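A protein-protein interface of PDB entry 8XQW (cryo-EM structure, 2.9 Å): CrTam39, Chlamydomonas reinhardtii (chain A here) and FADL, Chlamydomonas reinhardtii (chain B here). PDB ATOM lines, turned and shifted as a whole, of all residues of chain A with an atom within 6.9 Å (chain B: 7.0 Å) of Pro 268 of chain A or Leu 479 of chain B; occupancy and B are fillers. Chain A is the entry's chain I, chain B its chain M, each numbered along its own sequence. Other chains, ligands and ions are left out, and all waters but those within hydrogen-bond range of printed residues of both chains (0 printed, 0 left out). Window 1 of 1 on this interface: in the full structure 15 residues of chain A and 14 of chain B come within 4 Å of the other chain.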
ATOM      1  N   LEU A 256       9.635  -2.201   9.588  1.00  0.00           N
ATOM      2  CA  LEU A 256       8.707  -1.111   9.312  1.00  0.00           C
ATOM      3  C   LEU A 256       9.090   0.157  10.066  1.00  0.00           C
ATOM      4  O   LEU A 256       9.030   1.262   9.514  1.00  0.00           O
ATOM      5  CB  LEU A 256       7.296  -1.540   9.671  1.00  0.00           C
ATOM      6  CG  LEU A 256       6.210  -0.586   9.222  1.00  0.00           C
ATOM      7  CD1 LEU A 256       6.234  -0.463   7.727  1.00  0.00           C
ATOM      8  CD2 LEU A 256       4.898  -1.122   9.685  1.00  0.00           C
ATOM      9  N   ALA A 257       9.492   0.022  11.329  1.00  0.00           N
ATOM     10  CA  ALA A 257       9.899   1.200  12.088  1.00  0.00           C
ATOM     11  C   ALA A 257      11.164   1.820  11.520  1.00  0.00           C
ATOM     12  O   ALA A 257      11.284   3.046  11.453  1.00  0.00           O
ATOM     13  CB  ALA A 257      10.102   0.840  13.550  1.00  0.00           C
ATOM     14  N   ALA A 259      12.031   1.729   8.464  1.00  0.00           N
ATOM     15  CA  ALA A 259      11.672   2.409   7.229  1.00  0.00           C
ATOM     16  C   ALA A 259      11.085   3.774   7.520  1.00  0.00           C
ATOM     17  O   ALA A 259      11.453   4.762   6.881  1.00  0.00           O
ATOM     18  CB  ALA A 259      10.683   1.570   6.433  1.00  0.00           C
ATOM     19  N   ALA A 260      10.176   3.853   8.488  1.00  0.00           N
ATOM     20  CA  ALA A 260       9.597   5.144   8.834  1.00  0.00           C
ATOM     21  C   ALA A 260      10.631   6.099   9.402  1.00  0.00           C
ATOM     22  O   ALA A 260      10.474   7.313   9.281  1.00  0.00           O
ATOM     23  CB  ALA A 260       8.460   4.973   9.831  1.00  0.00           C
ATOM     24  N   MET A 261      11.677   5.589  10.015  1.00  0.00           N
ATOM     25  CA  MET A 261      12.689   6.453  10.620  1.00  0.00           C
ATOM     26  C   MET A 261      13.607   7.042   9.647  1.00  0.00           C
ATOM     27  O   MET A 261      14.628   7.531  10.074  1.00  0.00           O
ATOM     28  CB  MET A 261      13.498   5.672  11.649  1.00  0.00           C
ATOM     29  CG  MET A 261      13.128   5.971  13.062  1.00  0.00           C
ATOM     30  SD  MET A 261      14.238   5.238  14.266  1.00  0.00           S
ATOM     31  CE  MET A 261      14.250   3.559  13.713  1.00  0.00           C
ATOM     32  N   ASP A 263      13.001   9.640   7.730  1.00  0.00           N
ATOM     33  CA  ASP A 263      12.743  11.070   7.633  1.00  0.00           C
ATOM     34  C   ASP A 263      12.194  11.510   8.982  1.00  0.00           C
ATOM     35  O   ASP A 263      11.007  11.335   9.257  1.00  0.00           O
ATOM     36  CB  ASP A 263      11.777  11.386   6.512  1.00  0.00           C
ATOM     37  CG  ASP A 263      11.886  12.818   6.052  1.00  0.00           C
ATOM     38  OD1 ASP A 263      11.913  13.718   6.916  1.00  0.00           O
ATOM     39  OD2 ASP A 263      11.954  13.045   4.829  1.00  0.00           O
ATOM     40  N   ALA A 264      13.052  12.101   9.811  1.00  0.00           N
ATOM     41  CA  ALA A 264      12.729  12.279  11.217  1.00  0.00           C
ATOM     42  C   ALA A 264      11.917  13.533  11.495  1.00  0.00           C
ATOM     43  O   ALA A 264      11.488  13.736  12.634  1.00  0.00           O
ATOM     44  CB  ALA A 264      14.009  12.316  12.037  1.00  0.00           C
ATOM     45  N   ARG A 265      11.699  14.382  10.499  1.00  0.00           N
ATOM     46  CA  ARG A 265      10.978  15.621  10.754  1.00  0.00           C
ATOM     47  C   ARG A 265       9.473  15.415  10.694  1.00  0.00           C
ATOM     48  O   ARG A 265       8.716  16.165  11.316  1.00  0.00           O
ATOM     49  CB  ARG A 265      11.413  16.684   9.755  1.00  0.00           C
ATOM     50  CG  ARG A 265      12.904  16.909   9.728  1.00  0.00           C
ATOM     51  CD  ARG A 265      13.429  17.123  11.130  1.00  0.00           C
ATOM     52  NE  ARG A 265      14.518  18.091  11.167  1.00  0.00           N
ATOM     53  CZ  ARG A 265      15.798  17.785  10.985  1.00  0.00           C
ATOM     54  NH1 ARG A 265      16.720  18.731  11.038  1.00  0.00           N
ATOM     55  NH2 ARG A 265      16.154  16.533  10.749  1.00  0.00           N
ATOM     56  N   CYS A 266       9.020  14.404   9.961  1.00  0.00           N
ATOM     57  CA  CYS A 266       7.600  14.193   9.746  1.00  0.00           C
ATOM     58  C   CYS A 266       6.939  13.707  11.024  1.00  0.00           C
ATOM     59  O   CYS A 266       7.556  13.619  12.082  1.00  0.00           O
ATOM     60  CB  CYS A 266       7.386  13.183   8.633  1.00  0.00           C
ATOM     61  SG  CYS A 266       8.718  13.171   7.459  1.00  0.00           S
ATOM     62  N   VAL A 267       5.653  13.395  10.928  1.00  0.00           N
ATOM     63  CA  VAL A 267       4.940  12.736  12.014  1.00  0.00           C
ATOM     64  C   VAL A 267       5.221  11.235  11.971  1.00  0.00           C
ATOM     65  O   VAL A 267       5.518  10.639  13.022  1.00  0.00           O
ATOM     66  CB  VAL A 267       3.442  13.054  11.951  1.00  0.00           C
ATOM     67  CG1 VAL A 267       2.745  12.573  13.186  1.00  0.00           C
ATOM     68  CG2 VAL A 267       3.257  14.526  11.789  1.00  0.00           C
ATOM     69  N   PRO A 268       5.148  10.572  10.810  1.00  0.00           N
ATOM     70  CA  PRO A 268       5.601   9.178  10.766  1.00  0.00           C
ATOM     71  C   PRO A 268       7.028   8.993  11.234  1.00  0.00           C
ATOM     72  O   PRO A 268       7.353   7.936  11.785  1.00  0.00           O
ATOM     73  CB  PRO A 268       5.438   8.806   9.287  1.00  0.00           C
ATOM     74  CG  PRO A 268       5.177  10.053   8.584  1.00  0.00           C
ATOM     75  CD  PRO A 268       4.508  10.936   9.541  1.00  0.00           C
ATOM     76  N   GLY A 269       7.885   9.992  11.064  1.00  0.00           N
ATOM     77  CA  GLY A 269       9.245   9.865  11.550  1.00  0.00           C
ATOM     78  C   GLY A 269       9.323   9.713  13.055  1.00  0.00           C
ATOM     79  O   GLY A 269      10.308   9.203  13.584  1.00  0.00           O
ATOM     80  N   ALA A 270       8.292  10.163  13.765  1.00  0.00           N
ATOM     81  CA  ALA A 270       8.268  10.033  15.218  1.00  0.00           C
ATOM     82  C   ALA A 270       7.518   8.785  15.651  1.00  0.00           C
ATOM     83  O   ALA A 270       7.920   8.104  16.608  1.00  0.00           O
ATOM     84  CB  ALA A 270       7.635  11.270  15.843  1.00  0.00           C
ATOM     85  N   LEU A 271       6.425   8.468  14.967  1.00  0.00           N
ATOM     86  CA  LEU A 271       5.744   7.226  15.294  1.00  0.00           C
ATOM     87  C   LEU A 271       6.635   6.019  15.031  1.00  0.00           C
ATOM     88  O   LEU A 271       6.491   4.988  15.694  1.00  0.00           O
ATOM     89  CB  LEU A 271       4.441   7.130  14.519  1.00  0.00           C
ATOM     90  CG  LEU A 271       3.469   8.234  14.907  1.00  0.00           C
ATOM     91  CD1 LEU A 271       2.422   8.424  13.850  1.00  0.00           C
ATOM     92  CD2 LEU A 271       2.820   7.903  16.221  1.00  0.00           C
ATOM     93  N   GLY A 272       7.587   6.133  14.107  1.00  0.00           N
ATOM     94  CA  GLY A 272       8.529   5.044  13.914  1.00  0.00           C
ATOM     95  C   GLY A 272       9.367   4.772  15.144  1.00  0.00           C
ATOM     96  O   GLY A 272       9.520   3.626  15.568  1.00  0.00           O
ATOM     97  N   VAL A 273       9.939   5.822  15.723  1.00  0.00           N
ATOM     98  CA  VAL A 273      10.733   5.666  16.933  1.00  0.00           C
ATOM     99  C   VAL A 273       9.899   5.060  18.048  1.00  0.00           C
ATOM    100  O   VAL A 273      10.367   4.183  18.782  1.00  0.00           O
ATOM    101  CB  VAL A 273      11.312   7.019  17.352  1.00  0.00           C
ATOM    102  CG1 VAL A 273      12.270   6.828  18.467  1.00  0.00           C
ATOM    103  CG2 VAL A 273      11.993   7.663  16.200  1.00  0.00           C
ATOM    104  N   MET A 329       5.079  13.993  19.344  1.00  0.00           N
ATOM    105  CA  MET A 329       3.692  13.750  19.810  1.00  0.00           C
ATOM    106  C   MET A 329       3.615  13.925  21.327  1.00  0.00           C
ATOM    107  O   MET A 329       3.103  13.024  21.997  1.00  0.00           O
ATOM    108  CB  MET A 329       3.232  12.344  19.439  1.00  0.00           C
ATOM    109  CG  MET A 329       3.911  11.762  18.221  1.00  0.00           C
ATOM    110  SD  MET A 329       2.924  12.071  16.747  1.00  0.00           S
ATOM    111  CE  MET A 329       1.269  12.039  17.448  1.00  0.00           C
ATOM    112  N   SER B 390       5.147  -4.473  -3.479  1.00  0.00           N
ATOM    113  CA  SER B 390       4.362  -3.329  -3.039  1.00  0.00           C
ATOM    114  C   SER B 390       3.573  -2.766  -4.209  1.00  0.00           C
ATOM    115  O   SER B 390       4.097  -2.668  -5.318  1.00  0.00           O
ATOM    116  CB  SER B 390       5.263  -2.254  -2.455  1.00  0.00           C
ATOM    117  OG  SER B 390       4.576  -1.539  -1.456  1.00  0.00           O
ATOM    118  N   PRO B 392       1.938   0.512  -4.560  1.00  0.00           N
ATOM    119  CA  PRO B 392       2.305   1.859  -5.011  1.00  0.00           C
ATOM    120  C   PRO B 392       3.673   1.927  -5.650  1.00  0.00           C
ATOM    121  O   PRO B 392       3.843   2.585  -6.685  1.00  0.00           O
ATOM    122  CB  PRO B 392       2.247   2.672  -3.718  1.00  0.00           C
ATOM    123  CG  PRO B 392       1.386   1.909  -2.834  1.00  0.00           C
ATOM    124  CD  PRO B 392       1.687   0.501  -3.114  1.00  0.00           C
ATOM    125  N   LEU B 467      12.372   6.567   2.757  1.00  0.00           N
ATOM    126  CA  LEU B 467      11.316   7.511   2.435  1.00  0.00           C
ATOM    127  C   LEU B 467      11.845   8.803   1.854  1.00  0.00           C
ATOM    128  O   LEU B 467      11.067   9.739   1.676  1.00  0.00           O
ATOM    129  CB  LEU B 467      10.503   7.832   3.675  1.00  0.00           C
ATOM    130  CG  LEU B 467       9.436   6.842   4.079  1.00  0.00           C
ATOM    131  CD1 LEU B 467       8.799   7.340   5.324  1.00  0.00           C
ATOM    132  CD2 LEU B 467       8.436   6.732   2.986  1.00  0.00           C
ATOM    133  N   SER B 474       3.075  11.852  -0.049  1.00  0.00           N
ATOM    134  CA  SER B 474       2.676  10.475  -0.249  1.00  0.00           C
ATOM    135  C   SER B 474       3.208   9.517   0.795  1.00  0.00           C
ATOM    136  O   SER B 474       3.011   8.311   0.641  1.00  0.00           O
ATOM    137  CB  SER B 474       3.131   9.991  -1.620  1.00  0.00           C
ATOM    138  OG  SER B 474       4.524   9.848  -1.636  1.00  0.00           O
ATOM    139  N   TYR B 475       3.866  10.001   1.849  1.00  0.00           N
ATOM    140  CA  TYR B 475       4.532   9.091   2.773  1.00  0.00           C
ATOM    141  C   TYR B 475       3.575   8.037   3.296  1.00  0.00           C
ATOM    142  O   TYR B 475       3.839   6.840   3.181  1.00  0.00           O
ATOM    143  CB  TYR B 475       5.153   9.863   3.921  1.00  0.00           C
ATOM    144  CG  TYR B 475       6.452  10.494   3.548  1.00  0.00           C
ATOM    145  CD1 TYR B 475       7.023  10.245   2.330  1.00  0.00           C
ATOM    146  CD2 TYR B 475       7.110  11.329   4.410  1.00  0.00           C
ATOM    147  CE1 TYR B 475       8.191  10.809   1.980  1.00  0.00           C
ATOM    148  CE2 TYR B 475       8.287  11.895   4.066  1.00  0.00           C
ATOM    149  CZ  TYR B 475       8.825  11.632   2.849  1.00  0.00           C
ATOM    150  OH  TYR B 475      10.016  12.199   2.485  1.00  0.00           O
ATOM    151  N   VAL B 476       2.442   8.457   3.848  1.00  0.00           N
ATOM    152  CA  VAL B 476       1.514   7.503   4.437  1.00  0.00           C
ATOM    153  C   VAL B 476       1.079   6.460   3.422  1.00  0.00           C
ATOM    154  O   VAL B 476       0.882   5.295   3.771  1.00  0.00           O
ATOM    155  CB  VAL B 476       0.315   8.243   5.045  1.00  0.00           C
ATOM    156  CG1 VAL B 476      -0.797   7.294   5.342  1.00  0.00           C
ATOM    157  CG2 VAL B 476       0.739   8.931   6.302  1.00  0.00           C
ATOM    158  N   GLU B 477       0.948   6.836   2.155  1.00  0.00           N
ATOM    159  CA  GLU B 477       0.529   5.847   1.171  1.00  0.00           C
ATOM    160  C   GLU B 477       1.636   4.869   0.852  1.00  0.00           C
ATOM    161  O   GLU B 477       1.364   3.689   0.634  1.00  0.00           O
ATOM    162  CB  GLU B 477       0.072   6.513  -0.117  1.00  0.00           C
ATOM    163  CG  GLU B 477       0.424   5.708  -1.344  1.00  0.00           C
ATOM    164  CD  GLU B 477       0.003   6.357  -2.638  1.00  0.00           C
ATOM    165  OE1 GLU B 477      -0.939   5.844  -3.273  1.00  0.00           O
ATOM    166  OE2 GLU B 477       0.615   7.369  -3.029  1.00  0.00           O
ATOM    167  N   VAL B 478       2.882   5.329   0.829  1.00  0.00           N
ATOM    168  CA  VAL B 478       3.991   4.438   0.526  1.00  0.00           C
ATOM    169  C   VAL B 478       4.239   3.493   1.685  1.00  0.00           C
ATOM    170  O   VAL B 478       4.398   2.285   1.495  1.00  0.00           O
ATOM    171  CB  VAL B 478       5.246   5.246   0.183  1.00  0.00           C
ATOM    172  CG1 VAL B 478       6.433   4.380   0.278  1.00  0.00           C
ATOM    173  CG2 VAL B 478       5.125   5.782  -1.202  1.00  0.00           C
ATOM    174  N   LEU B 479       4.255   4.022   2.906  1.00  0.00           N
ATOM    175  CA  LEU B 479       4.448   3.182   4.078  1.00  0.00           C
ATOM    176  C   LEU B 479       3.431   2.060   4.122  1.00  0.00           C
ATOM    177  O   LEU B 479       3.791   0.894   4.285  1.00  0.00           O
ATOM    178  CB  LEU B 479       4.361   4.021   5.346  1.00  0.00           C
ATOM    179  CG  LEU B 479       5.627   4.732   5.786  1.00  0.00           C
ATOM    180  CD1 LEU B 479       5.300   5.734   6.854  1.00  0.00           C
ATOM    181  CD2 LEU B 479       6.610   3.739   6.300  1.00  0.00           C
ATOM    182  N   SER B 480       2.150   2.391   3.973  1.00  0.00           N
ATOM    183  CA  SER B 480       1.121   1.357   3.929  1.00  0.00           C
ATOM    184  C   SER B 480       1.446   0.308   2.882  1.00  0.00           C
ATOM    185  O   SER B 480       1.289  -0.891   3.124  1.00  0.00           O
ATOM    186  CB  SER B 480      -0.241   1.972   3.641  1.00  0.00           C
ATOM    187  OG  SER B 480      -0.504   3.052   4.506  1.00  0.00           O
ATOM    188  N   GLY B 481       1.933   0.734   1.726  1.00  0.00           N
ATOM    189  CA  GLY B 481       2.285  -0.219   0.699  1.00  0.00           C
ATOM    190  C   GLY B 481       3.331  -1.209   1.147  1.00  0.00           C
ATOM    191  O   GLY B 481       3.266  -2.379   0.787  1.00  0.00           O
ATOM    192  N   TRP B 482       4.307  -0.762   1.929  1.00  0.00           N
ATOM    193  CA  TRP B 482       5.345  -1.663   2.403  1.00  0.00           C
ATOM    194  C   TRP B 482       4.870  -2.546   3.531  1.00  0.00           C
ATOM    195  O   TRP B 482       5.546  -3.519   3.857  1.00  0.00           O
ATOM    196  CB  TRP B 482       6.556  -0.893   2.904  1.00  0.00           C
ATOM    197  CG  TRP B 482       7.409  -0.335   1.867  1.00  0.00           C
ATOM    198  CD1 TRP B 482       7.619  -0.830   0.632  1.00  0.00           C
ATOM    199  CD2 TRP B 482       8.197   0.841   1.968  1.00  0.00           C
ATOM    200  NE1 TRP B 482       8.486  -0.034  -0.054  1.00  0.00           N
ATOM    201  CE2 TRP B 482       8.861   1.002   0.754  1.00  0.00           C
ATOM    202  CE3 TRP B 482       8.406   1.777   2.977  1.00  0.00           C
ATOM    203  CZ2 TRP B 482       9.709   2.057   0.514  1.00  0.00           C
ATOM    204  CZ3 TRP B 482       9.252   2.818   2.737  1.00  0.00           C
ATOM    205  CH2 TRP B 482       9.891   2.953   1.517  1.00  0.00           C
ATOM    206  N   ALA B 483       3.746  -2.226   4.152  1.00  0.00           N
ATOM    207  CA  ALA B 483       3.348  -2.983   5.322  1.00  0.00           C
ATOM    208  C   ALA B 483       2.536  -4.206   4.971  1.00  0.00           C
ATOM    209  O   ALA B 483       2.328  -5.054   5.834  1.00  0.00           O
ATOM    210  CB  ALA B 483       2.559  -2.102   6.279  1.00  0.00           C
ATOM    211  N   ALA B 484       2.070  -4.321   3.746  1.00  0.00           N
ATOM    212  CA  ALA B 484       1.312  -5.499   3.365  1.00  0.00           C
ATOM    213  C   ALA B 484       2.237  -6.666   3.040  1.00  0.00           C
ATOM    214  O   ALA B 484       1.971  -7.782   3.493  1.00  0.00           O
ATOM    215  CB  ALA B 484       0.383  -5.183   2.198  1.00  0.00           C
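Printed residues of chain B within 4 Å of Asp 263 of chain A: Tyr 475.
Ala 264 of chain A touches none of the printed residues of chain B.
Printed residues of chain B within 4 Å of Cys 266 of chain A: Tyr 475.
Printed residues of chain B within 4 Å of Pro 268 of chain A: Leu 479.
Of the printed residues of chain A, Tyr 475 of chain B touches Asp 263 (3.2 Å) and Cys 266 (3.7 Å).
Of the printed residues of chain A, Leu 479 of chain B touches Pro 268.
The nearest residue of chain B that does not touch Pro 268 of chain A is Tyr 475 of chain B (4.7 Å).
The nearest residue of chain A that does not touch Leu 479 of chain B is Ala 260 of chain A (4.2 Å).
The side-chain hydroxyl of Tyr 475 of chain B lies within hydrogen-bond range of the side-chain carboxylate of Asp 263 of chain A, 3.2 Å away.
The side-chain carboxylate of Asp 263 of chain A lies within hydrogen-bond range of the side-chain sulfur of Cys 266 of chain A (3.3 Å).
O of Leu 467 of chain B sits at hydrogen-bond distance from OH of Tyr 475 of chain B (2.8 Å).
Of the 14 printed residues of chain B, 2 touch a printed residue of chain A.
Printed residues of chain B that touch a printed residue of chain A: Tyr 475 and Leu 479.
Of the 17 printed residues of chain A, 3 touch a printed residue of chain B.
Among the printed residues, 3 pairs touch across the chains.
Among the printed residues, no Asp or Glu carboxylate lies within 4 Å of a Lys or Arg side-chain nitrogen of the other chain.
Among the printed residues, merely in contact across the chains: Cys 266 of chain A with Tyr 475 of chain B (3.7 Å) and Pro 268 of chain A with Leu 479 of chain B (3.9 Å).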
